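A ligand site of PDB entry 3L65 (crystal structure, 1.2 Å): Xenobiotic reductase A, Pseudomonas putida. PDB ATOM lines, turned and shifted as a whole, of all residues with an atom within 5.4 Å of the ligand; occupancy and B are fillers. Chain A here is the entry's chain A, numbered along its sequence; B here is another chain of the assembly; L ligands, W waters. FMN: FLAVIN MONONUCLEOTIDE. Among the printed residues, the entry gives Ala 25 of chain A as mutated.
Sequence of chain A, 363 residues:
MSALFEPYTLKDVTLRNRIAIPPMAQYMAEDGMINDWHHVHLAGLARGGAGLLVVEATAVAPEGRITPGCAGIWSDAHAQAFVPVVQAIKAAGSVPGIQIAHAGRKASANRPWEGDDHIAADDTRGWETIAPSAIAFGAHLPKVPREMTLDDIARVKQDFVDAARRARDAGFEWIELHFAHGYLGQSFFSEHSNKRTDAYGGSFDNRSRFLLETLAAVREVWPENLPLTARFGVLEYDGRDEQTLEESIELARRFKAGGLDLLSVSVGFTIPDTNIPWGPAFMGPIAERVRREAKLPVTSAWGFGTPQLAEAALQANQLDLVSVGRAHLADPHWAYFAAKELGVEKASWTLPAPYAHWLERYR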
ATOM      1  N   PRO A  22      10.666   3.748  -5.693  1.00  0.00           N
ATOM      2  CA  PRO A  22       9.514   2.893  -5.974  1.00  0.00           C
ATOM      3  C   PRO A  22       8.354   3.791  -6.425  1.00  0.00           C
ATOM      4  O   PRO A  22       8.354   5.008  -6.182  1.00  0.00           O
ATOM      5  CB  PRO A  22       9.233   2.213  -4.625  1.00  0.00           C
ATOM      6  CG  PRO A  22       9.671   3.257  -3.624  1.00  0.00           C
ATOM      7  CD  PRO A  22      10.886   3.914  -4.244  1.00  0.00           C
ATOM      8  N   PRO A  23       7.321   3.171  -7.009  1.00  0.00           N
ATOM      9  CA  PRO A  23       6.126   3.942  -7.402  1.00  0.00           C
ATOM     10  C   PRO A  23       5.538   4.627  -6.171  1.00  0.00           C
ATOM     11  O   PRO A  23       5.318   4.007  -5.132  1.00  0.00           O
ATOM     12  CB  PRO A  23       5.199   2.863  -8.013  1.00  0.00           C
ATOM     13  CG  PRO A  23       5.708   1.567  -7.388  1.00  0.00           C
ATOM     14  CD  PRO A  23       7.178   1.729  -7.265  1.00  0.00           C
ATOM     15  N   MET A  24       5.242   5.908  -6.347  1.00  0.00           N
ATOM     16  CA  MET A  24       4.569   6.673  -5.295  1.00  0.00           C
ATOM     17  C   MET A  24       3.504   7.584  -5.914  1.00  0.00           C
ATOM     18  O   MET A  24       3.817   8.646  -6.459  1.00  0.00           O
ATOM     19  CB  MET A  24       5.576   7.529  -4.500  1.00  0.00           C
ATOM     20  CG  MET A  24       6.444   6.688  -3.566  1.00  0.00           C
ATOM     21  SD  MET A  24       7.614   7.676  -2.571  1.00  0.00           S
ATOM     22  CE  MET A  24       8.790   8.061  -3.844  1.00  0.00           C
ATOM     23  N   ALA A  25       2.262   7.156  -5.775  1.00  0.00           N
ATOM     24  CA  ALA A  25       1.111   7.925  -6.191  1.00  0.00           C
ATOM     25  C   ALA A  25       1.187   9.358  -5.688  1.00  0.00           C
ATOM     26  O   ALA A  25       1.490   9.619  -4.531  1.00  0.00           O
ATOM     27  CB  ALA A  25      -0.136   7.267  -5.679  1.00  0.00           C
ATOM     28  N   GLN A  26       0.853  10.286  -6.592  1.00  0.00           N
ATOM     29  CA  GLN A  26       0.887  11.721  -6.329  1.00  0.00           C
ATOM     30  C   GLN A  26      -0.499  12.354  -6.194  1.00  0.00           C
ATOM     31  O   GLN A  26      -0.596  13.470  -5.664  1.00  0.00           O
ATOM     32  CB  GLN A  26       1.685  12.444  -7.411  1.00  0.00           C
ATOM     33  CG  GLN A  26       3.137  12.002  -7.457  1.00  0.00           C
ATOM     34  CD  GLN A  26       3.870  12.405  -6.196  1.00  0.00           C
ATOM     35  OE1 GLN A  26       4.166  13.577  -5.983  1.00  0.00           O
ATOM     36  NE2 GLN A  26       4.177  11.412  -5.316  1.00  0.00           N
ATOM     37  N   TYR A  27      -1.515  11.692  -6.716  1.00  0.00           N
ATOM     38  CA  TYR A  27      -2.901  12.156  -6.606  1.00  0.00           C
ATOM     39  C   TYR A  27      -3.105  13.535  -7.237  1.00  0.00           C
ATOM     40  O   TYR A  27      -3.968  14.285  -6.787  1.00  0.00           O
ATOM     41  CB  TYR A  27      -3.405  12.101  -5.147  1.00  0.00           C
ATOM     42  CG  TYR A  27      -3.094  10.772  -4.467  1.00  0.00           C
ATOM     43  CD1 TYR A  27      -3.969   9.718  -4.553  1.00  0.00           C
ATOM     44  CD2 TYR A  27      -1.920  10.578  -3.756  1.00  0.00           C
ATOM     45  CE1 TYR A  27      -3.716   8.501  -3.956  1.00  0.00           C
ATOM     46  CE2 TYR A  27      -1.653   9.368  -3.152  1.00  0.00           C
ATOM     47  CZ  TYR A  27      -2.552   8.338  -3.244  1.00  0.00           C
ATOM     48  OH  TYR A  27      -2.241   7.147  -2.602  1.00  0.00           O
ATOM     49  N   GLU A  56       4.557   6.163 -10.471  1.00  0.00           N
ATOM     50  CA  GLU A  56       3.433   5.779  -9.654  1.00  0.00           C
ATOM     51  C   GLU A  56       2.428   4.870 -10.372  1.00  0.00           C
ATOM     52  O   GLU A  56       2.293   4.894 -11.605  1.00  0.00           O
ATOM     53  CB  GLU A  56       2.668   7.042  -9.243  1.00  0.00           C
ATOM     54  CG  GLU A  56       2.032   7.839 -10.425  1.00  0.00           C
ATOM     55  CD  GLU A  56       1.670   9.245  -9.964  1.00  0.00           C
ATOM     56  OE1 GLU A  56       0.547   9.426  -9.432  1.00  0.00           O
ATOM     57  OE2 GLU A  56       2.506  10.151 -10.140  1.00  0.00           O
ATOM     58  N   ALA A  57       1.644   4.155  -9.555  1.00  0.00           N
ATOM     59  CA  ALA A  57       0.522   3.336 -10.025  1.00  0.00           C
ATOM     60  C   ALA A  57      -0.273   4.124 -11.075  1.00  0.00           C
ATOM     61  O   ALA A  57      -0.906   5.118 -10.752  1.00  0.00           O
ATOM     62  CB  ALA A  57      -0.374   2.992  -8.869  1.00  0.00           C
ATOM     63  N   GLN A  99       4.715   1.683 -13.138  1.00  0.00           N
ATOM     64  CA  GLN A  99       3.872   0.677 -12.561  1.00  0.00           C
ATOM     65  C   GLN A  99       2.480   0.819 -13.143  1.00  0.00           C
ATOM     66  O   GLN A  99       1.885   1.869 -13.019  1.00  0.00           O
ATOM     67  CB  GLN A  99       3.824   0.824 -11.019  1.00  0.00           C
ATOM     68  CG  GLN A  99       3.058  -0.290 -10.344  1.00  0.00           C
ATOM     69  CD  GLN A  99       2.822  -0.024  -8.878  1.00  0.00           C
ATOM     70  OE1 GLN A  99       2.212   0.973  -8.532  1.00  0.00           O
ATOM     71  NE2 GLN A  99       3.312  -0.928  -7.999  1.00  0.00           N
ATOM     72  N   GLU A 176       6.388  -2.492 -14.313  1.00  0.00           N
ATOM     73  CA  GLU A 176       6.019  -3.191 -13.094  1.00  0.00           C
ATOM     74  C   GLU A 176       4.512  -3.394 -13.060  1.00  0.00           C
ATOM     75  O   GLU A 176       3.741  -2.441 -13.076  1.00  0.00           O
ATOM     76  CB  GLU A 176       6.468  -2.410 -11.861  1.00  0.00           C
ATOM     77  CG  GLU A 176       6.261  -3.146 -10.537  1.00  0.00           C
ATOM     78  CD  GLU A 176       6.664  -2.334  -9.332  1.00  0.00           C
ATOM     79  OE1 GLU A 176       7.847  -2.099  -9.098  1.00  0.00           O
ATOM     80  OE2 GLU A 176       5.772  -1.911  -8.588  1.00  0.00           O
ATOM     81  N   HIS A 178       1.274  -4.126 -11.060  1.00  0.00           N
ATOM     82  CA  HIS A 178       0.908  -3.914  -9.666  1.00  0.00           C
ATOM     83  C   HIS A 178      -0.011  -5.018  -9.186  1.00  0.00           C
ATOM     84  O   HIS A 178      -1.260  -4.909  -9.210  1.00  0.00           O
ATOM     85  CB  HIS A 178       0.258  -2.562  -9.462  1.00  0.00           C
ATOM     86  CG  HIS A 178       0.204  -2.152  -8.030  1.00  0.00           C
ATOM     87  ND1 HIS A 178       0.553  -3.001  -6.991  1.00  0.00           N
ATOM     88  CD2 HIS A 178      -0.043  -0.939  -7.474  1.00  0.00           C
ATOM     89  CE1 HIS A 178       0.511  -2.313  -5.856  1.00  0.00           C
ATOM     90  NE2 HIS A 178       0.161  -1.063  -6.115  1.00  0.00           N
ATOM     91  N   HIS A 181      -0.719  -5.002  -2.553  1.00  0.00           N
ATOM     92  CA  HIS A 181      -1.380  -3.962  -1.776  1.00  0.00           C
ATOM     93  C   HIS A 181      -2.894  -4.019  -1.820  1.00  0.00           C
ATOM     94  O   HIS A 181      -3.570  -3.033  -1.603  1.00  0.00           O
ATOM     95  CB  HIS A 181      -0.842  -2.581  -2.134  1.00  0.00           C
ATOM     96  CG  HIS A 181       0.644  -2.470  -1.951  1.00  0.00           C
ATOM     97  ND1 HIS A 181       1.367  -1.417  -2.460  1.00  0.00           N
ATOM     98  CD2 HIS A 181       1.528  -3.252  -1.283  1.00  0.00           C
ATOM     99  CE1 HIS A 181       2.648  -1.569  -2.121  1.00  0.00           C
ATOM    100  NE2 HIS A 181       2.766  -2.681  -1.424  1.00  0.00           N
ATOM    101  N   ARG A 231       5.086  -6.240  -8.711  1.00  0.00           N
ATOM    102  CA  ARG A 231       5.046  -6.058  -7.268  1.00  0.00           C
ATOM    103  C   ARG A 231       3.971  -6.975  -6.739  1.00  0.00           C
ATOM    104  O   ARG A 231       2.879  -7.060  -7.301  1.00  0.00           O
ATOM    105  CB  ARG A 231       4.763  -4.597  -6.901  1.00  0.00           C
ATOM    106  CG  ARG A 231       5.162  -4.274  -5.426  1.00  0.00           C
ATOM    107  CD  ARG A 231       5.150  -2.816  -5.079  1.00  0.00           C
ATOM    108  NE  ARG A 231       6.121  -2.581  -3.993  1.00  0.00           N
ATOM    109  CZ  ARG A 231       6.394  -1.392  -3.470  1.00  0.00           C
ATOM    110  NH1 ARG A 231       7.367  -1.272  -2.569  1.00  0.00           N
ATOM    111  NH2 ARG A 231       5.680  -0.333  -3.831  1.00  0.00           N
ATOM    112  N   ALA A 301      11.080  -2.556   0.247  1.00  0.00           N
ATOM    113  CA  ALA A 301      11.002  -1.193   0.742  1.00  0.00           C
ATOM    114  C   ALA A 301      10.571  -1.236   2.191  1.00  0.00           C
ATOM    115  O   ALA A 301      10.176  -2.299   2.684  1.00  0.00           O
ATOM    116  CB  ALA A 301       9.996  -0.340  -0.088  1.00  0.00           C
ATOM    117  N   TRP A 302      10.714  -0.088   2.837  1.00  0.00           N
ATOM    118  CA  TRP A 302      10.196   0.309   4.152  1.00  0.00           C
ATOM    119  C   TRP A 302      11.365   0.543   5.073  1.00  0.00           C
ATOM    120  O   TRP A 302      11.909  -0.388   5.681  1.00  0.00           O
ATOM    121  CB  TRP A 302       9.176  -0.612   4.790  1.00  0.00           C
ATOM    122  CG  TRP A 302       8.608   0.051   6.017  1.00  0.00           C
ATOM    123  CD1 TRP A 302       9.181   0.137   7.287  1.00  0.00           C
ATOM    124  CD2 TRP A 302       7.397   0.783   6.089  1.00  0.00           C
ATOM    125  NE1 TRP A 302       8.354   0.833   8.127  1.00  0.00           N
ATOM    126  CE2 TRP A 302       7.269   1.261   7.412  1.00  0.00           C
ATOM    127  CE3 TRP A 302       6.395   1.057   5.175  1.00  0.00           C
ATOM    128  CZ2 TRP A 302       6.163   2.019   7.823  1.00  0.00           C
ATOM    129  CZ3 TRP A 302       5.306   1.814   5.577  1.00  0.00           C
ATOM    130  CH2 TRP A 302       5.195   2.281   6.890  1.00  0.00           C
ATOM    131  N   GLY A 303      11.738   1.820   5.204  1.00  0.00           N
ATOM    132  CA  GLY A 303      12.798   2.223   6.112  1.00  0.00           C
ATOM    133  C   GLY A 303      14.213   2.166   5.590  1.00  0.00           C
ATOM    134  O   GLY A 303      15.150   2.288   6.373  1.00  0.00           O
ATOM    135  N   PHE A 304      14.417   1.990   4.295  1.00  0.00           N
ATOM    136  CA  PHE A 304      15.770   1.974   3.755  1.00  0.00           C
ATOM    137  C   PHE A 304      16.382   3.343   3.483  1.00  0.00           C
ATOM    138  O   PHE A 304      17.480   3.444   2.935  1.00  0.00           O
ATOM    139  CB  PHE A 304      15.837   1.074   2.516  1.00  0.00           C
ATOM    140  CG  PHE A 304      15.637  -0.384   2.817  1.00  0.00           C
ATOM    141  CD1 PHE A 304      16.674  -1.127   3.362  1.00  0.00           C
ATOM    142  CD2 PHE A 304      14.423  -1.018   2.545  1.00  0.00           C
ATOM    143  CE1 PHE A 304      16.520  -2.471   3.608  1.00  0.00           C
ATOM    144  CE2 PHE A 304      14.246  -2.372   2.813  1.00  0.00           C
ATOM    145  CZ  PHE A 304      15.306  -3.107   3.359  1.00  0.00           C
ATOM    146  N   GLY A 305      15.695   4.402   3.892  1.00  0.00           N
ATOM    147  CA  GLY A 305      16.263   5.735   3.826  1.00  0.00           C
ATOM    148  C   GLY A 305      17.431   5.996   4.764  1.00  0.00           C
ATOM    149  O   GLY A 305      18.095   7.027   4.654  1.00  0.00           O
ATOM    150  N   SER A 323      14.698  -0.112  -2.597  1.00  0.00           N
ATOM    151  CA  SER A 323      13.701   0.886  -2.912  1.00  0.00           C
ATOM    152  C   SER A 323      13.583   1.853  -1.736  1.00  0.00           C
ATOM    153  O   SER A 323      13.385   1.428  -0.586  1.00  0.00           O
ATOM    154  CB  SER A 323      12.362   0.228  -3.185  1.00  0.00           C
ATOM    155  OG  SER A 323      12.417  -0.532  -4.399  1.00  0.00           O
ATOM    156  N   VAL A 324      13.671   3.144  -2.041  1.00  0.00           N
ATOM    157  CA  VAL A 324      13.688   4.215  -1.055  1.00  0.00           C
ATOM    158  C   VAL A 324      12.616   5.239  -1.476  1.00  0.00           C
ATOM    159  O   VAL A 324      12.764   5.953  -2.470  1.00  0.00           O
ATOM    160  CB  VAL A 324      15.078   4.863  -0.969  1.00  0.00           C
ATOM    161  CG1 VAL A 324      15.062   6.028   0.031  1.00  0.00           C
ATOM    162  CG2 VAL A 324      16.151   3.818  -0.610  1.00  0.00           C
ATOM    163  N   GLY A 325      11.515   5.270  -0.727  1.00  0.00           N
ATOM    164  CA  GLY A 325      10.324   6.032  -1.067  1.00  0.00           C
ATOM    165  C   GLY A 325      10.259   7.383  -0.366  1.00  0.00           C
ATOM    166  O   GLY A 325      10.641   8.418  -0.928  1.00  0.00           O
ATOM    167  N   ARG A 326       9.743   7.385   0.862  1.00  0.00           N
ATOM    168  CA  ARG A 326       9.500   8.659   1.554  1.00  0.00           C
ATOM    169  C   ARG A 326      10.731   9.530   1.721  1.00  0.00           C
ATOM    170  O   ARG A 326      10.605  10.759   1.666  1.00  0.00           O
ATOM    171  CB  ARG A 326       8.834   8.406   2.913  1.00  0.00           C
ATOM    172  CG  ARG A 326       7.376   8.030   2.772  1.00  0.00           C
ATOM    173  CD  ARG A 326       6.771   7.488   4.038  1.00  0.00           C
ATOM    174  NE  ARG A 326       7.338   6.176   4.313  1.00  0.00           N
ATOM    175  CZ  ARG A 326       7.018   5.445   5.365  1.00  0.00           C
ATOM    176  NH1 ARG A 326       6.127   5.903   6.218  1.00  0.00           N
ATOM    177  NH2 ARG A 326       7.595   4.275   5.576  1.00  0.00           N
ATOM    178  N   ALA A 327      11.915   8.958   1.891  1.00  0.00           N
ATOM    179  CA  ALA A 327      13.102   9.773   2.000  1.00  0.00           C
ATOM    180  C   ALA A 327      13.330  10.629   0.749  1.00  0.00           C
ATOM    181  O   ALA A 327      13.933  11.703   0.870  1.00  0.00           O
ATOM    182  CB  ALA A 327      14.319   8.934   2.288  1.00  0.00           C
ATOM    183  N   LEU A 329      10.741  11.907  -1.076  1.00  0.00           N
ATOM    184  CA  LEU A 329       9.798  12.994  -0.956  1.00  0.00           C
ATOM    185  C   LEU A 329      10.386  14.088  -0.085  1.00  0.00           C
ATOM    186  O   LEU A 329      10.273  15.263  -0.397  1.00  0.00           O
ATOM    187  CB  LEU A 329       8.432  12.535  -0.435  1.00  0.00           C
ATOM    188  CG  LEU A 329       7.809  11.332  -1.164  1.00  0.00           C
ATOM    189  CD1 LEU A 329       6.505  10.966  -0.505  1.00  0.00           C
ATOM    190  CD2 LEU A 329       7.627  11.598  -2.673  1.00  0.00           C
ATOM    191  N   PRO B 354       1.188  16.381  -1.714  1.00  0.00           N
ATOM    192  CA  PRO B 354       1.619  15.017  -2.109  1.00  0.00           C
ATOM    193  C   PRO B 354       2.918  14.580  -1.456  1.00  0.00           C
ATOM    194  O   PRO B 354       3.257  13.391  -1.518  1.00  0.00           O
ATOM    195  CB  PRO B 354       1.807  15.111  -3.621  1.00  0.00           C
ATOM    196  CG  PRO B 354       0.924  16.294  -4.043  1.00  0.00           C
ATOM    197  CD  PRO B 354       0.987  17.261  -2.887  1.00  0.00           C
ATOM    198  N   TRP B 358       2.648  12.575   3.864  1.00  0.00           N
ATOM    199  CA  TRP B 358       3.357  11.339   4.188  1.00  0.00           C
ATOM    200  C   TRP B 358       4.534  11.537   5.131  1.00  0.00           C
ATOM    201  O   TRP B 358       5.088  10.591   5.629  1.00  0.00           O
ATOM    202  CB  TRP B 358       3.880  10.713   2.889  1.00  0.00           C
ATOM    203  CG  TRP B 358       2.821  10.594   1.928  1.00  0.00           C
ATOM    204  CD1 TRP B 358       2.624  11.406   0.863  1.00  0.00           C
ATOM    205  CD2 TRP B 358       1.747   9.673   1.945  1.00  0.00           C
ATOM    206  NE1 TRP B 358       1.484  11.038   0.194  1.00  0.00           N
ATOM    207  CE2 TRP B 358       0.926   9.963   0.833  1.00  0.00           C
ATOM    208  CE3 TRP B 358       1.387   8.621   2.799  1.00  0.00           C
ATOM    209  CZ2 TRP B 358      -0.203   9.251   0.537  1.00  0.00           C
ATOM    210  CZ3 TRP B 358       0.249   7.909   2.507  1.00  0.00           C
ATOM    211  CH2 TRP B 358      -0.538   8.219   1.371  1.00  0.00           C
ATOM    212  N   TYR B 362       7.584  12.364  10.389  1.00  0.00           N
ATOM    213  CA  TYR B 362       8.524  11.452   9.730  1.00  0.00           C
ATOM    214  C   TYR B 362       9.959  11.845  10.045  1.00  0.00           C
ATOM    215  O   TYR B 362      10.376  12.968   9.747  1.00  0.00           O
ATOM    216  CB  TYR B 362       8.295  11.459   8.222  1.00  0.00           C
ATOM    217  CG  TYR B 362       9.141  10.451   7.475  1.00  0.00           C
ATOM    218  CD1 TYR B 362      10.343  10.831   6.880  1.00  0.00           C
ATOM    219  CD2 TYR B 362       8.752   9.119   7.385  1.00  0.00           C
ATOM    220  CE1 TYR B 362      11.124   9.913   6.196  1.00  0.00           C
ATOM    221  CE2 TYR B 362       9.531   8.181   6.697  1.00  0.00           C
ATOM    222  CZ  TYR B 362      10.714   8.594   6.107  1.00  0.00           C
ATOM    223  OH  TYR B 362      11.477   7.677   5.432  1.00  0.00           O
HETATM  224  N1  FMN L   1       3.357   1.541  -3.716  1.00  0.00           N
HETATM  225  C2  FMN L   1       3.015   1.058  -4.925  1.00  0.00           C
HETATM  226  O2  FMN L   1       3.171  -0.143  -5.217  1.00  0.00           O
HETATM  227  N3  FMN L   1       2.417   1.931  -5.837  1.00  0.00           N
HETATM  228  C4  FMN L   1       2.163   3.234  -5.598  1.00  0.00           C
HETATM  229  O4  FMN L   1       1.762   3.992  -6.529  1.00  0.00           O
HETATM  230  C4A FMN L   1       2.404   3.637  -4.312  1.00  0.00           C
HETATM  231  N5  FMN L   1       2.047   4.944  -3.942  1.00  0.00           N
HETATM  232  C5A FMN L   1       2.657   5.475  -2.740  1.00  0.00           C
HETATM  233  C6  FMN L   1       2.543   6.854  -2.519  1.00  0.00           C
HETATM  234  C7  FMN L   1       3.232   7.442  -1.434  1.00  0.00           C
HETATM  235  C7M FMN L   1       3.300   8.980  -1.404  1.00  0.00           C
HETATM  236  C8  FMN L   1       3.945   6.594  -0.584  1.00  0.00           C
HETATM  237  C8M FMN L   1       4.711   7.284   0.576  1.00  0.00           C
HETATM  238  C9  FMN L   1       4.018   5.278  -0.783  1.00  0.00           C
HETATM  239  C9A FMN L   1       3.410   4.685  -1.908  1.00  0.00           C
HETATM  240  N10 FMN L   1       3.575   3.293  -2.226  1.00  0.00           N
HETATM  241  C10 FMN L   1       3.093   2.807  -3.423  1.00  0.00           C
HETATM  242  C1' FMN L   1       4.545   2.470  -1.359  1.00  0.00           C
HETATM  243  C2' FMN L   1       5.954   2.865  -1.632  1.00  0.00           C
HETATM  244  O2' FMN L   1       6.345   2.405  -2.968  1.00  0.00           O
HETATM  245  C3' FMN L   1       6.940   2.193  -0.639  1.00  0.00           C
HETATM  246  O3' FMN L   1       6.854   0.761  -0.672  1.00  0.00           O
HETATM  247  C4' FMN L   1       6.724   2.647   0.847  1.00  0.00           C
HETATM  248  O4' FMN L   1       6.599   4.087   0.883  1.00  0.00           O
HETATM  249  C5' FMN L   1       7.785   2.095   1.796  1.00  0.00           C
HETATM  250  O5' FMN L   1       9.095   2.668   1.508  1.00  0.00           O
HETATM  251  P   FMN L   1       9.698   3.918   2.349  1.00  0.00           P
HETATM  252  O1P FMN L   1       8.756   5.057   2.128  1.00  0.00           O
HETATM  253  O2P FMN L   1       9.733   3.534   3.825  1.00  0.00           O
HETATM  254  O3P FMN L   1      11.009   4.097   1.770  1.00  0.00           O
HETATM  255  O   HOH W   1      12.496   6.263   2.595  1.00  0.00           O
HETATM  256  O   HOH W   2       4.345   4.315   2.952  1.00  0.00           O
HETATM  257  O   HOH W   3      10.815   5.220   5.661  1.00  0.00           O
HETATM  258  O   HOH W   4       2.062   0.855   0.215  1.00  0.00           O
HETATM  259  O   HOH W   5      12.533   1.900   1.997  1.00  0.00           O
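O3P of the ligand sits at hydrogen-bond distance from N of Gly 325 (2.8 Å). O3' of the ligand lies within hydrogen-bond range of NH1 of Arg 231. An oxygen (O1P) of the ligand sits at hydrogen-bond distance from the backbone NH of Arg 326, at 2.8 Å. NE of Arg 326 lies within salt-bridge range of O1P of the ligand (2.8 Å). N3 of the ligand is in hydrogen-bond range of OE1 of Gln 99, at 2.9 Å. A nitrogen (N5) of the ligand sits at hydrogen-bond distance from the backbone NH (N) of Ala 25 (2.9 Å). The backbone carbonyl oxygen (O) of Pro 23 is in hydrogen-bond range of an oxygen (O2') of the ligand, 2.9 Å away. The backbone NH of Gly 303 sits at hydrogen-bond distance from an oxygen (O2P) of the ligand (3.0 Å). The backbone NH (N) of Ala 57 lies within hydrogen-bond range of an oxygen (O4) of the ligand (3.0 Å). A ring nitrogen (NE2) of His 178 lies within hydrogen-bond range of an oxygen (O2) of the ligand, 3.3 Å away. The backbone NH of Trp 302 is in hydrogen-bond range of an oxygen (O5') of the ligand, 3.5 Å away.
The side-chain amide oxygen of Gln 99 sits close to the backbone NH of Ala 57, at 3.4 Å. The side-chain amide nitrogen (NE2) of Gln 99 sits at hydrogen-bond distance from the side-chain carboxylate (OE2) of Glu 176, at 2.7 Å. O of Pro 354 of chain B lies close to NE1 of Trp 358 of chain B, 3.4 Å away. The backbone carbonyl oxygen (O) of Met 24 sits at hydrogen-bond distance from the side-chain amide nitrogen (NE2) of Gln 26. OE1 of Glu 56 lies within hydrogen-bond range of N of Gln 26, at 3.0 Å.
Pro 22 touches the ligand. Met 24 touches the ligand. CA of Glu 56 touches O4 of the ligand, at 3.97 Å. His 181 touches the ligand (CE1 to O2, 3.4 Å). Ala 301 touches the ligand. Val 324 touches the ligand. CD1 of Leu 329 touches C7M of the ligand, 3.9 Å away. Trp 358 of chain B touches the ligand. The nearest printed residue that does not touch the ligand is Ser 323 (4.3 Å).
Water W3 lies within hydrogen-bond range of the side-chain hydroxyl (OH) of Tyr 362 of chain B (2.6 Å), an oxygen (O2P) of the ligand (2.7 Å) and the guanidinium group (NH2) of Arg 326 (3.4 Å). Water W1 lies within hydrogen-bond range of an oxygen (O3P) of the ligand (2.8 Å), the backbone NH of Ala 327 (2.8 Å), the side-chain hydroxyl of Tyr 362 of chain B (3.3 Å) and the backbone NH of Arg 326 (3.4 Å).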
